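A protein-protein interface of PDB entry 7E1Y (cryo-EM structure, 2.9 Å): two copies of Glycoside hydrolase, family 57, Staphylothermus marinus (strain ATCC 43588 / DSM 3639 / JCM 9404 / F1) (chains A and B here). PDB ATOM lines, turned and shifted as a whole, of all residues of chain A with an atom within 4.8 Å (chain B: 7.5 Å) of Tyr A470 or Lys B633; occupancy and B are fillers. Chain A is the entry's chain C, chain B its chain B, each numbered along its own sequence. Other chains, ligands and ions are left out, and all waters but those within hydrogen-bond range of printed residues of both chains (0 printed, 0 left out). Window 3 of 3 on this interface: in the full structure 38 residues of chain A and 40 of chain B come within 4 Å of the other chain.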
ATOM      1  N   LEU A 249      25.148 -12.240 -20.757  1.00  0.00           N
ATOM      2  CA  LEU A 249      26.407 -11.514 -20.879  1.00  0.00           C
ATOM      3  C   LEU A 249      27.117 -11.804 -22.194  1.00  0.00           C
ATOM      4  O   LEU A 249      27.695 -10.888 -22.788  1.00  0.00           O
ATOM      5  CB  LEU A 249      27.332 -11.846 -19.707  1.00  0.00           C
ATOM      6  CG  LEU A 249      26.922 -11.323 -18.329  1.00  0.00           C
ATOM      7  CD1 LEU A 249      27.889 -11.810 -17.263  1.00  0.00           C
ATOM      8  CD2 LEU A 249      26.861  -9.808 -18.331  1.00  0.00           C
ATOM      9  N   TRP A 466      25.225  -5.984 -11.719  1.00  0.00           N
ATOM     10  CA  TRP A 466      25.405  -6.651 -13.000  1.00  0.00           C
ATOM     11  C   TRP A 466      25.894  -5.685 -14.065  1.00  0.00           C
ATOM     12  O   TRP A 466      26.792  -6.027 -14.840  1.00  0.00           O
ATOM     13  CB  TRP A 466      24.100  -7.306 -13.455  1.00  0.00           C
ATOM     14  CG  TRP A 466      23.903  -8.692 -12.927  1.00  0.00           C
ATOM     15  CD1 TRP A 466      22.899  -9.121 -12.115  1.00  0.00           C
ATOM     16  CD2 TRP A 466      24.745  -9.826 -13.156  1.00  0.00           C
ATOM     17  NE1 TRP A 466      23.055 -10.453 -11.831  1.00  0.00           N
ATOM     18  CE2 TRP A 466      24.184 -10.909 -12.457  1.00  0.00           C
ATOM     19  CE3 TRP A 466      25.917 -10.032 -13.886  1.00  0.00           C
ATOM     20  CZ2 TRP A 466      24.751 -12.177 -12.468  1.00  0.00           C
ATOM     21  CZ3 TRP A 466      26.479 -11.287 -13.893  1.00  0.00           C
ATOM     22  CH2 TRP A 466      25.898 -12.346 -13.190  1.00  0.00           C
ATOM     23  N   ILE A 467      25.334  -4.475 -14.104  1.00  0.00           N
ATOM     24  CA  ILE A 467      25.821  -3.472 -15.044  1.00  0.00           C
ATOM     25  C   ILE A 467      27.264  -3.106 -14.721  1.00  0.00           C
ATOM     26  O   ILE A 467      28.081  -2.886 -15.622  1.00  0.00           O
ATOM     27  CB  ILE A 467      24.897  -2.242 -15.031  1.00  0.00           C
ATOM     28  CG1 ILE A 467      23.608  -2.546 -15.793  1.00  0.00           C
ATOM     29  CG2 ILE A 467      25.584  -1.041 -15.650  1.00  0.00           C
ATOM     30  CD1 ILE A 467      22.620  -1.411 -15.796  1.00  0.00           C
ATOM     31  N   LYS A 468      27.607  -3.074 -13.432  1.00  0.00           N
ATOM     32  CA  LYS A 468      28.965  -2.731 -13.025  1.00  0.00           C
ATOM     33  C   LYS A 468      29.970  -3.780 -13.488  1.00  0.00           C
ATOM     34  O   LYS A 468      31.000  -3.446 -14.097  1.00  0.00           O
ATOM     35  CB  LYS A 468      29.008  -2.562 -11.507  1.00  0.00           C
ATOM     36  CG  LYS A 468      30.388  -2.382 -10.917  1.00  0.00           C
ATOM     37  CD  LYS A 468      30.329  -2.420  -9.401  1.00  0.00           C
ATOM     38  CE  LYS A 468      29.206  -1.544  -8.870  1.00  0.00           C
ATOM     39  NZ  LYS A 468      29.373  -1.232  -7.426  1.00  0.00           N
ATOM     40  N   THR A 469      29.691  -5.056 -13.216  1.00  0.00           N
ATOM     41  CA  THR A 469      30.601  -6.102 -13.665  1.00  0.00           C
ATOM     42  C   THR A 469      30.641  -6.221 -15.188  1.00  0.00           C
ATOM     43  O   THR A 469      31.705  -6.521 -15.746  1.00  0.00           O
ATOM     44  CB  THR A 469      30.236  -7.447 -13.025  1.00  0.00           C
ATOM     45  OG1 THR A 469      31.116  -8.467 -13.511  1.00  0.00           O
ATOM     46  CG2 THR A 469      28.820  -7.835 -13.344  1.00  0.00           C
ATOM     47  N   TYR A 470      29.527  -5.957 -15.876  1.00  0.00           N
ATOM     48  CA  TYR A 470      29.526  -5.935 -17.330  1.00  0.00           C
ATOM     49  C   TYR A 470      30.374  -4.806 -17.896  1.00  0.00           C
ATOM     50  O   TYR A 470      31.072  -5.010 -18.896  1.00  0.00           O
ATOM     51  CB  TYR A 470      28.091  -5.815 -17.846  1.00  0.00           C
ATOM     52  CG  TYR A 470      27.952  -5.953 -19.340  1.00  0.00           C
ATOM     53  CD1 TYR A 470      28.751  -6.830 -20.050  1.00  0.00           C
ATOM     54  CD2 TYR A 470      27.005  -5.222 -20.037  1.00  0.00           C
ATOM     55  CE1 TYR A 470      28.622  -6.963 -21.413  1.00  0.00           C
ATOM     56  CE2 TYR A 470      26.870  -5.350 -21.398  1.00  0.00           C
ATOM     57  CZ  TYR A 470      27.681  -6.221 -22.081  1.00  0.00           C
ATOM     58  OH  TYR A 470      27.549  -6.353 -23.441  1.00  0.00           O
ATOM     59  N   SER A 471      30.341  -3.629 -17.268  1.00  0.00           N
ATOM     60  CA  SER A 471      31.231  -2.547 -17.664  1.00  0.00           C
ATOM     61  C   SER A 471      32.689  -2.920 -17.448  1.00  0.00           C
ATOM     62  O   SER A 471      33.532  -2.644 -18.309  1.00  0.00           O
ATOM     63  CB  SER A 471      30.890  -1.279 -16.885  1.00  0.00           C
ATOM     64  OG  SER A 471      29.723  -0.669 -17.395  1.00  0.00           O
ATOM     65  N   VAL A 472      33.001  -3.551 -16.313  1.00  0.00           N
ATOM     66  CA  VAL A 472      34.376  -3.985 -16.074  1.00  0.00           C
ATOM     67  C   VAL A 472      34.832  -4.977 -17.138  1.00  0.00           C
ATOM     68  O   VAL A 472      35.966  -4.895 -17.619  1.00  0.00           O
ATOM     69  CB  VAL A 472      34.518  -4.582 -14.664  1.00  0.00           C
ATOM     70  CG1 VAL A 472      35.851  -5.280 -14.512  1.00  0.00           C
ATOM     71  CG2 VAL A 472      34.371  -3.502 -13.614  1.00  0.00           C
ATOM     72  N   TYR A 473      33.974  -5.919 -17.525  1.00  0.00           N
ATOM     73  CA  TYR A 473      34.339  -6.885 -18.558  1.00  0.00           C
ATOM     74  C   TYR A 473      34.505  -6.243 -19.931  1.00  0.00           C
ATOM     75  O   TYR A 473      35.420  -6.611 -20.684  1.00  0.00           O
ATOM     76  CB  TYR A 473      33.289  -7.991 -18.628  1.00  0.00           C
ATOM     77  CG  TYR A 473      33.437  -8.900 -19.821  1.00  0.00           C
ATOM     78  CD1 TYR A 473      34.489  -9.796 -19.907  1.00  0.00           C
ATOM     79  CD2 TYR A 473      32.525  -8.861 -20.860  1.00  0.00           C
ATOM     80  CE1 TYR A 473      34.628 -10.627 -20.993  1.00  0.00           C
ATOM     81  CE2 TYR A 473      32.655  -9.688 -21.951  1.00  0.00           C
ATOM     82  CZ  TYR A 473      33.709 -10.568 -22.012  1.00  0.00           C
ATOM     83  OH  TYR A 473      33.844 -11.399 -23.099  1.00  0.00           O
ATOM     84  N   ARG A 474      33.629  -5.285 -20.251  1.00  0.00           N
ATOM     85  CA  ARG A 474      33.700  -4.574 -21.556  1.00  0.00           C
ATOM     86  C   ARG A 474      35.036  -3.828 -21.617  1.00  0.00           C
ATOM     87  O   ARG A 474      35.669  -3.829 -22.689  1.00  0.00           O
ATOM     88  CB  ARG A 474      32.512  -3.618 -21.711  1.00  0.00           C
ATOM     89  CG  ARG A 474      31.180  -4.323 -21.921  1.00  0.00           C
ATOM     90  CD  ARG A 474      30.232  -3.509 -22.780  1.00  0.00           C
ATOM     91  NE  ARG A 474      30.751  -3.328 -24.127  1.00  0.00           N
ATOM     92  CZ  ARG A 474      30.145  -2.627 -25.079  1.00  0.00           C
ATOM     93  NH1 ARG A 474      28.989  -2.037 -24.833  1.00  0.00           N
ATOM     94  NH2 ARG A 474      30.698  -2.519 -26.274  1.00  0.00           N
ATOM     95  N   PHE B 545      21.258   7.036 -19.201  1.00  0.00           N
ATOM     96  CA  PHE B 545      21.598   6.745 -20.588  1.00  0.00           C
ATOM     97  C   PHE B 545      22.107   5.320 -20.733  1.00  0.00           C
ATOM     98  O   PHE B 545      22.920   4.861 -19.927  1.00  0.00           O
ATOM     99  CB  PHE B 545      22.649   7.726 -21.104  1.00  0.00           C
ATOM    100  CG  PHE B 545      22.070   8.913 -21.800  1.00  0.00           C
ATOM    101  CD1 PHE B 545      21.610   9.997 -21.081  1.00  0.00           C
ATOM    102  CD2 PHE B 545      21.972   8.940 -23.175  1.00  0.00           C
ATOM    103  CE1 PHE B 545      21.075  11.088 -21.722  1.00  0.00           C
ATOM    104  CE2 PHE B 545      21.436  10.029 -23.817  1.00  0.00           C
ATOM    105  CZ  PHE B 545      20.987  11.104 -23.088  1.00  0.00           C
ATOM    106  N   TYR B 546      21.628   4.632 -21.769  1.00  0.00           N
ATOM    107  CA  TYR B 546      22.063   3.286 -22.110  1.00  0.00           C
ATOM    108  C   TYR B 546      22.505   3.262 -23.564  1.00  0.00           C
ATOM    109  O   TYR B 546      22.005   4.036 -24.384  1.00  0.00           O
ATOM    110  CB  TYR B 546      20.951   2.260 -21.883  1.00  0.00           C
ATOM    111  CG  TYR B 546      20.641   2.035 -20.427  1.00  0.00           C
ATOM    112  CD1 TYR B 546      21.534   1.366 -19.606  1.00  0.00           C
ATOM    113  CD2 TYR B 546      19.467   2.508 -19.867  1.00  0.00           C
ATOM    114  CE1 TYR B 546      21.264   1.168 -18.274  1.00  0.00           C
ATOM    115  CE2 TYR B 546      19.188   2.316 -18.534  1.00  0.00           C
ATOM    116  CZ  TYR B 546      20.090   1.642 -17.742  1.00  0.00           C
ATOM    117  OH  TYR B 546      19.821   1.443 -16.409  1.00  0.00           O
ATOM    118  N   GLU B 547      23.442   2.370 -23.875  1.00  0.00           N
ATOM    119  CA  GLU B 547      24.033   2.329 -25.204  1.00  0.00           C
ATOM    120  C   GLU B 547      22.999   1.951 -26.253  1.00  0.00           C
ATOM    121  O   GLU B 547      22.347   0.909 -26.160  1.00  0.00           O
ATOM    122  CB  GLU B 547      25.188   1.330 -25.233  1.00  0.00           C
ATOM    123  CG  GLU B 547      25.998   1.353 -26.513  1.00  0.00           C
ATOM    124  CD  GLU B 547      26.990   0.212 -26.583  1.00  0.00           C
ATOM    125  OE1 GLU B 547      26.765  -0.810 -25.904  1.00  0.00           O
ATOM    126  OE2 GLU B 547      28.001   0.339 -27.306  1.00  0.00           O
ATOM    127  N   ASP B 548      22.864   2.809 -27.261  1.00  0.00           N
ATOM    128  CA  ASP B 548      21.971   2.595 -28.396  1.00  0.00           C
ATOM    129  C   ASP B 548      20.533   2.364 -27.939  1.00  0.00           C
ATOM    130  O   ASP B 548      19.787   1.562 -28.505  1.00  0.00           O
ATOM    131  CB  ASP B 548      22.470   1.442 -29.268  1.00  0.00           C
ATOM    132  CG  ASP B 548      23.451   1.899 -30.323  1.00  0.00           C
ATOM    133  OD1 ASP B 548      23.167   2.912 -30.995  1.00  0.00           O
ATOM    134  OD2 ASP B 548      24.512   1.258 -30.470  1.00  0.00           O
ATOM    135  N   GLU B 549      20.150   3.090 -26.889  1.00  0.00           N
ATOM    136  CA  GLU B 549      18.766   3.072 -26.425  1.00  0.00           C
ATOM    137  C   GLU B 549      18.322   4.531 -26.311  1.00  0.00           C
ATOM    138  O   GLU B 549      19.090   5.378 -25.847  1.00  0.00           O
ATOM    139  CB  GLU B 549      18.620   2.332 -25.105  1.00  0.00           C
ATOM    140  CG  GLU B 549      17.203   2.366 -24.563  1.00  0.00           C
ATOM    141  CD  GLU B 549      17.102   1.853 -23.144  1.00  0.00           C
ATOM    142  OE1 GLU B 549      16.038   2.042 -22.517  1.00  0.00           O
ATOM    143  OE2 GLU B 549      18.077   1.246 -22.660  1.00  0.00           O
ATOM    144  N   ILE B 605      29.856   3.592 -25.032  1.00  0.00           N
ATOM    145  CA  ILE B 605      29.728   3.598 -23.582  1.00  0.00           C
ATOM    146  C   ILE B 605      30.966   4.266 -23.007  1.00  0.00           C
ATOM    147  O   ILE B 605      32.035   4.244 -23.622  1.00  0.00           O
ATOM    148  CB  ILE B 605      29.553   2.179 -23.002  1.00  0.00           C
ATOM    149  CG1 ILE B 605      30.727   1.286 -23.386  1.00  0.00           C
ATOM    150  CG2 ILE B 605      28.265   1.564 -23.485  1.00  0.00           C
ATOM    151  CD1 ILE B 605      30.977   0.175 -22.404  1.00  0.00           C
ATOM    152  N   VAL B 630      27.340   7.002 -20.163  1.00  0.00           N
ATOM    153  CA  VAL B 630      26.451   6.058 -20.826  1.00  0.00           C
ATOM    154  C   VAL B 630      26.793   4.648 -20.369  1.00  0.00           C
ATOM    155  O   VAL B 630      27.950   4.220 -20.435  1.00  0.00           O
ATOM    156  CB  VAL B 630      26.559   6.196 -22.353  1.00  0.00           C
ATOM    157  CG1 VAL B 630      25.692   5.170 -23.039  1.00  0.00           C
ATOM    158  CG2 VAL B 630      26.162   7.591 -22.780  1.00  0.00           C
ATOM    159  N   LYS B 631      25.783   3.920 -19.897  1.00  0.00           N
ATOM    160  CA  LYS B 631      26.017   2.588 -19.372  1.00  0.00           C
ATOM    161  C   LYS B 631      25.637   1.523 -20.394  1.00  0.00           C
ATOM    162  O   LYS B 631      24.741   1.734 -21.215  1.00  0.00           O
ATOM    163  CB  LYS B 631      25.227   2.357 -18.078  1.00  0.00           C
ATOM    164  CG  LYS B 631      25.679   3.226 -16.925  1.00  0.00           C
ATOM    165  CD  LYS B 631      24.873   2.940 -15.674  1.00  0.00           C
ATOM    166  CE  LYS B 631      25.390   3.746 -14.496  1.00  0.00           C
ATOM    167  NZ  LYS B 631      25.165   5.206 -14.683  1.00  0.00           N
ATOM    168  N   PRO B 632      26.308   0.373 -20.377  1.00  0.00           N
ATOM    169  CA  PRO B 632      25.967  -0.692 -21.325  1.00  0.00           C
ATOM    170  C   PRO B 632      24.579  -1.246 -21.060  1.00  0.00           C
ATOM    171  O   PRO B 632      24.175  -1.451 -19.913  1.00  0.00           O
ATOM    172  CB  PRO B 632      27.043  -1.758 -21.075  1.00  0.00           C
ATOM    173  CG  PRO B 632      28.032  -1.145 -20.153  1.00  0.00           C
ATOM    174  CD  PRO B 632      27.346  -0.050 -19.428  1.00  0.00           C
ATOM    175  N   LYS B 633      23.849  -1.494 -22.138  1.00  0.00           N
ATOM    176  CA  LYS B 633      22.533  -2.104 -22.031  1.00  0.00           C
ATOM    177  C   LYS B 633      22.711  -3.606 -21.860  1.00  0.00           C
ATOM    178  O   LYS B 633      23.380  -4.253 -22.670  1.00  0.00           O
ATOM    179  CB  LYS B 633      21.693  -1.787 -23.262  1.00  0.00           C
ATOM    180  CG  LYS B 633      20.284  -2.341 -23.212  1.00  0.00           C
ATOM    181  CD  LYS B 633      19.469  -1.653 -22.133  1.00  0.00           C
ATOM    182  CE  LYS B 633      18.057  -2.208 -22.060  1.00  0.00           C
ATOM    183  NZ  LYS B 633      17.273  -1.900 -23.289  1.00  0.00           N
ATOM    184  N   LEU B 634      22.121  -4.158 -20.806  1.00  0.00           N
ATOM    185  CA  LEU B 634      22.292  -5.564 -20.475  1.00  0.00           C
ATOM    186  C   LEU B 634      21.002  -6.324 -20.755  1.00  0.00           C
ATOM    187  O   LEU B 634      19.911  -5.881 -20.380  1.00  0.00           O
ATOM    188  CB  LEU B 634      22.701  -5.730 -19.011  1.00  0.00           C
ATOM    189  CG  LEU B 634      23.096  -7.147 -18.605  1.00  0.00           C
ATOM    190  CD1 LEU B 634      24.254  -7.620 -19.461  1.00  0.00           C
ATOM    191  CD2 LEU B 634      23.459  -7.201 -17.133  1.00  0.00           C
ATOM    192  N   LEU B 635      21.136  -7.468 -21.417  1.00  0.00           N
ATOM    193  CA  LEU B 635      19.994  -8.244 -21.877  1.00  0.00           C
ATOM    194  C   LEU B 635      19.238  -8.845 -20.700  1.00  0.00           C
ATOM    195  O   LEU B 635      19.814  -9.140 -19.651  1.00  0.00           O
ATOM    196  CB  LEU B 635      20.470  -9.336 -22.832  1.00  0.00           C
ATOM    197  CG  LEU B 635      21.050  -8.860 -24.166  1.00  0.00           C
ATOM    198  CD1 LEU B 635      21.614 -10.033 -24.954  1.00  0.00           C
ATOM    199  CD2 LEU B 635      20.000  -8.118 -24.977  1.00  0.00           C
ATOM    200  N   PRO B 636      17.930  -9.042 -20.844  1.00  0.00           N
ATOM    201  CA  PRO B 636      17.140  -9.655 -19.774  1.00  0.00           C
ATOM    202  C   PRO B 636      17.358 -11.159 -19.686  1.00  0.00           C
ATOM    203  O   PRO B 636      17.988 -11.780 -20.545  1.00  0.00           O
ATOM    204  CB  PRO B 636      15.695  -9.335 -20.182  1.00  0.00           C
ATOM    205  CG  PRO B 636      15.748  -9.240 -21.664  1.00  0.00           C
ATOM    206  CD  PRO B 636      17.096  -8.655 -21.996  1.00  0.00           C
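OE1 of Glu B547 lies within salt-bridge range of NH1 of Arg A474 (2.8 Å).
The backbone carbonyl oxygen of Lys B631 sits at hydrogen-bond distance from the backbone NH of Glu B547, 3.0 Å away. The side-chain carboxylate of Glu B549 lies within salt-bridge range of the side-chain amino group of Lys B633 (3.3 Å). The backbone carbonyl oxygen of Ile A467 sits at hydrogen-bond distance from the side-chain hydroxyl of Ser A471 (3.3 Å).
No position is printed for both chains.
Of the 10 printed residues of chain A, 6 touch a printed residue of chain B. Hydrophobic or aromatic side chains of chain A within 4 Å of the printed part of chain B: Leu A249, Trp A466, Ile A467 and Tyr A470. Of the 13 printed residues of chain B, 6 touch a printed residue of chain A. Among the printed residues, Asp or Glu carboxylates within 4 Å of a Lys or Arg side-chain nitrogen of the other chain: Arg A474 with Glu B547 (2.8 Å).
Among the printed residues, pairs that only touch across the chains: Leu A249 with Leu B634, Trp A466 with Leu B634, Ile A467 with Tyr B546, Tyr A470 with Pro B632, Tyr A470 with Lys B633, Tyr A470 with Leu B634, Ser A471 with Pro B632 and Arg A474 with Ile B605.
Printed residues of chain B within 4 Å of Leu A249: Leu B634 (3.6 Å). Printed residues of chain B within 4 Å of Trp A466: Leu B634 (3.7 Å). Lys B633 touches just one residue of chain A: Tyr A470.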
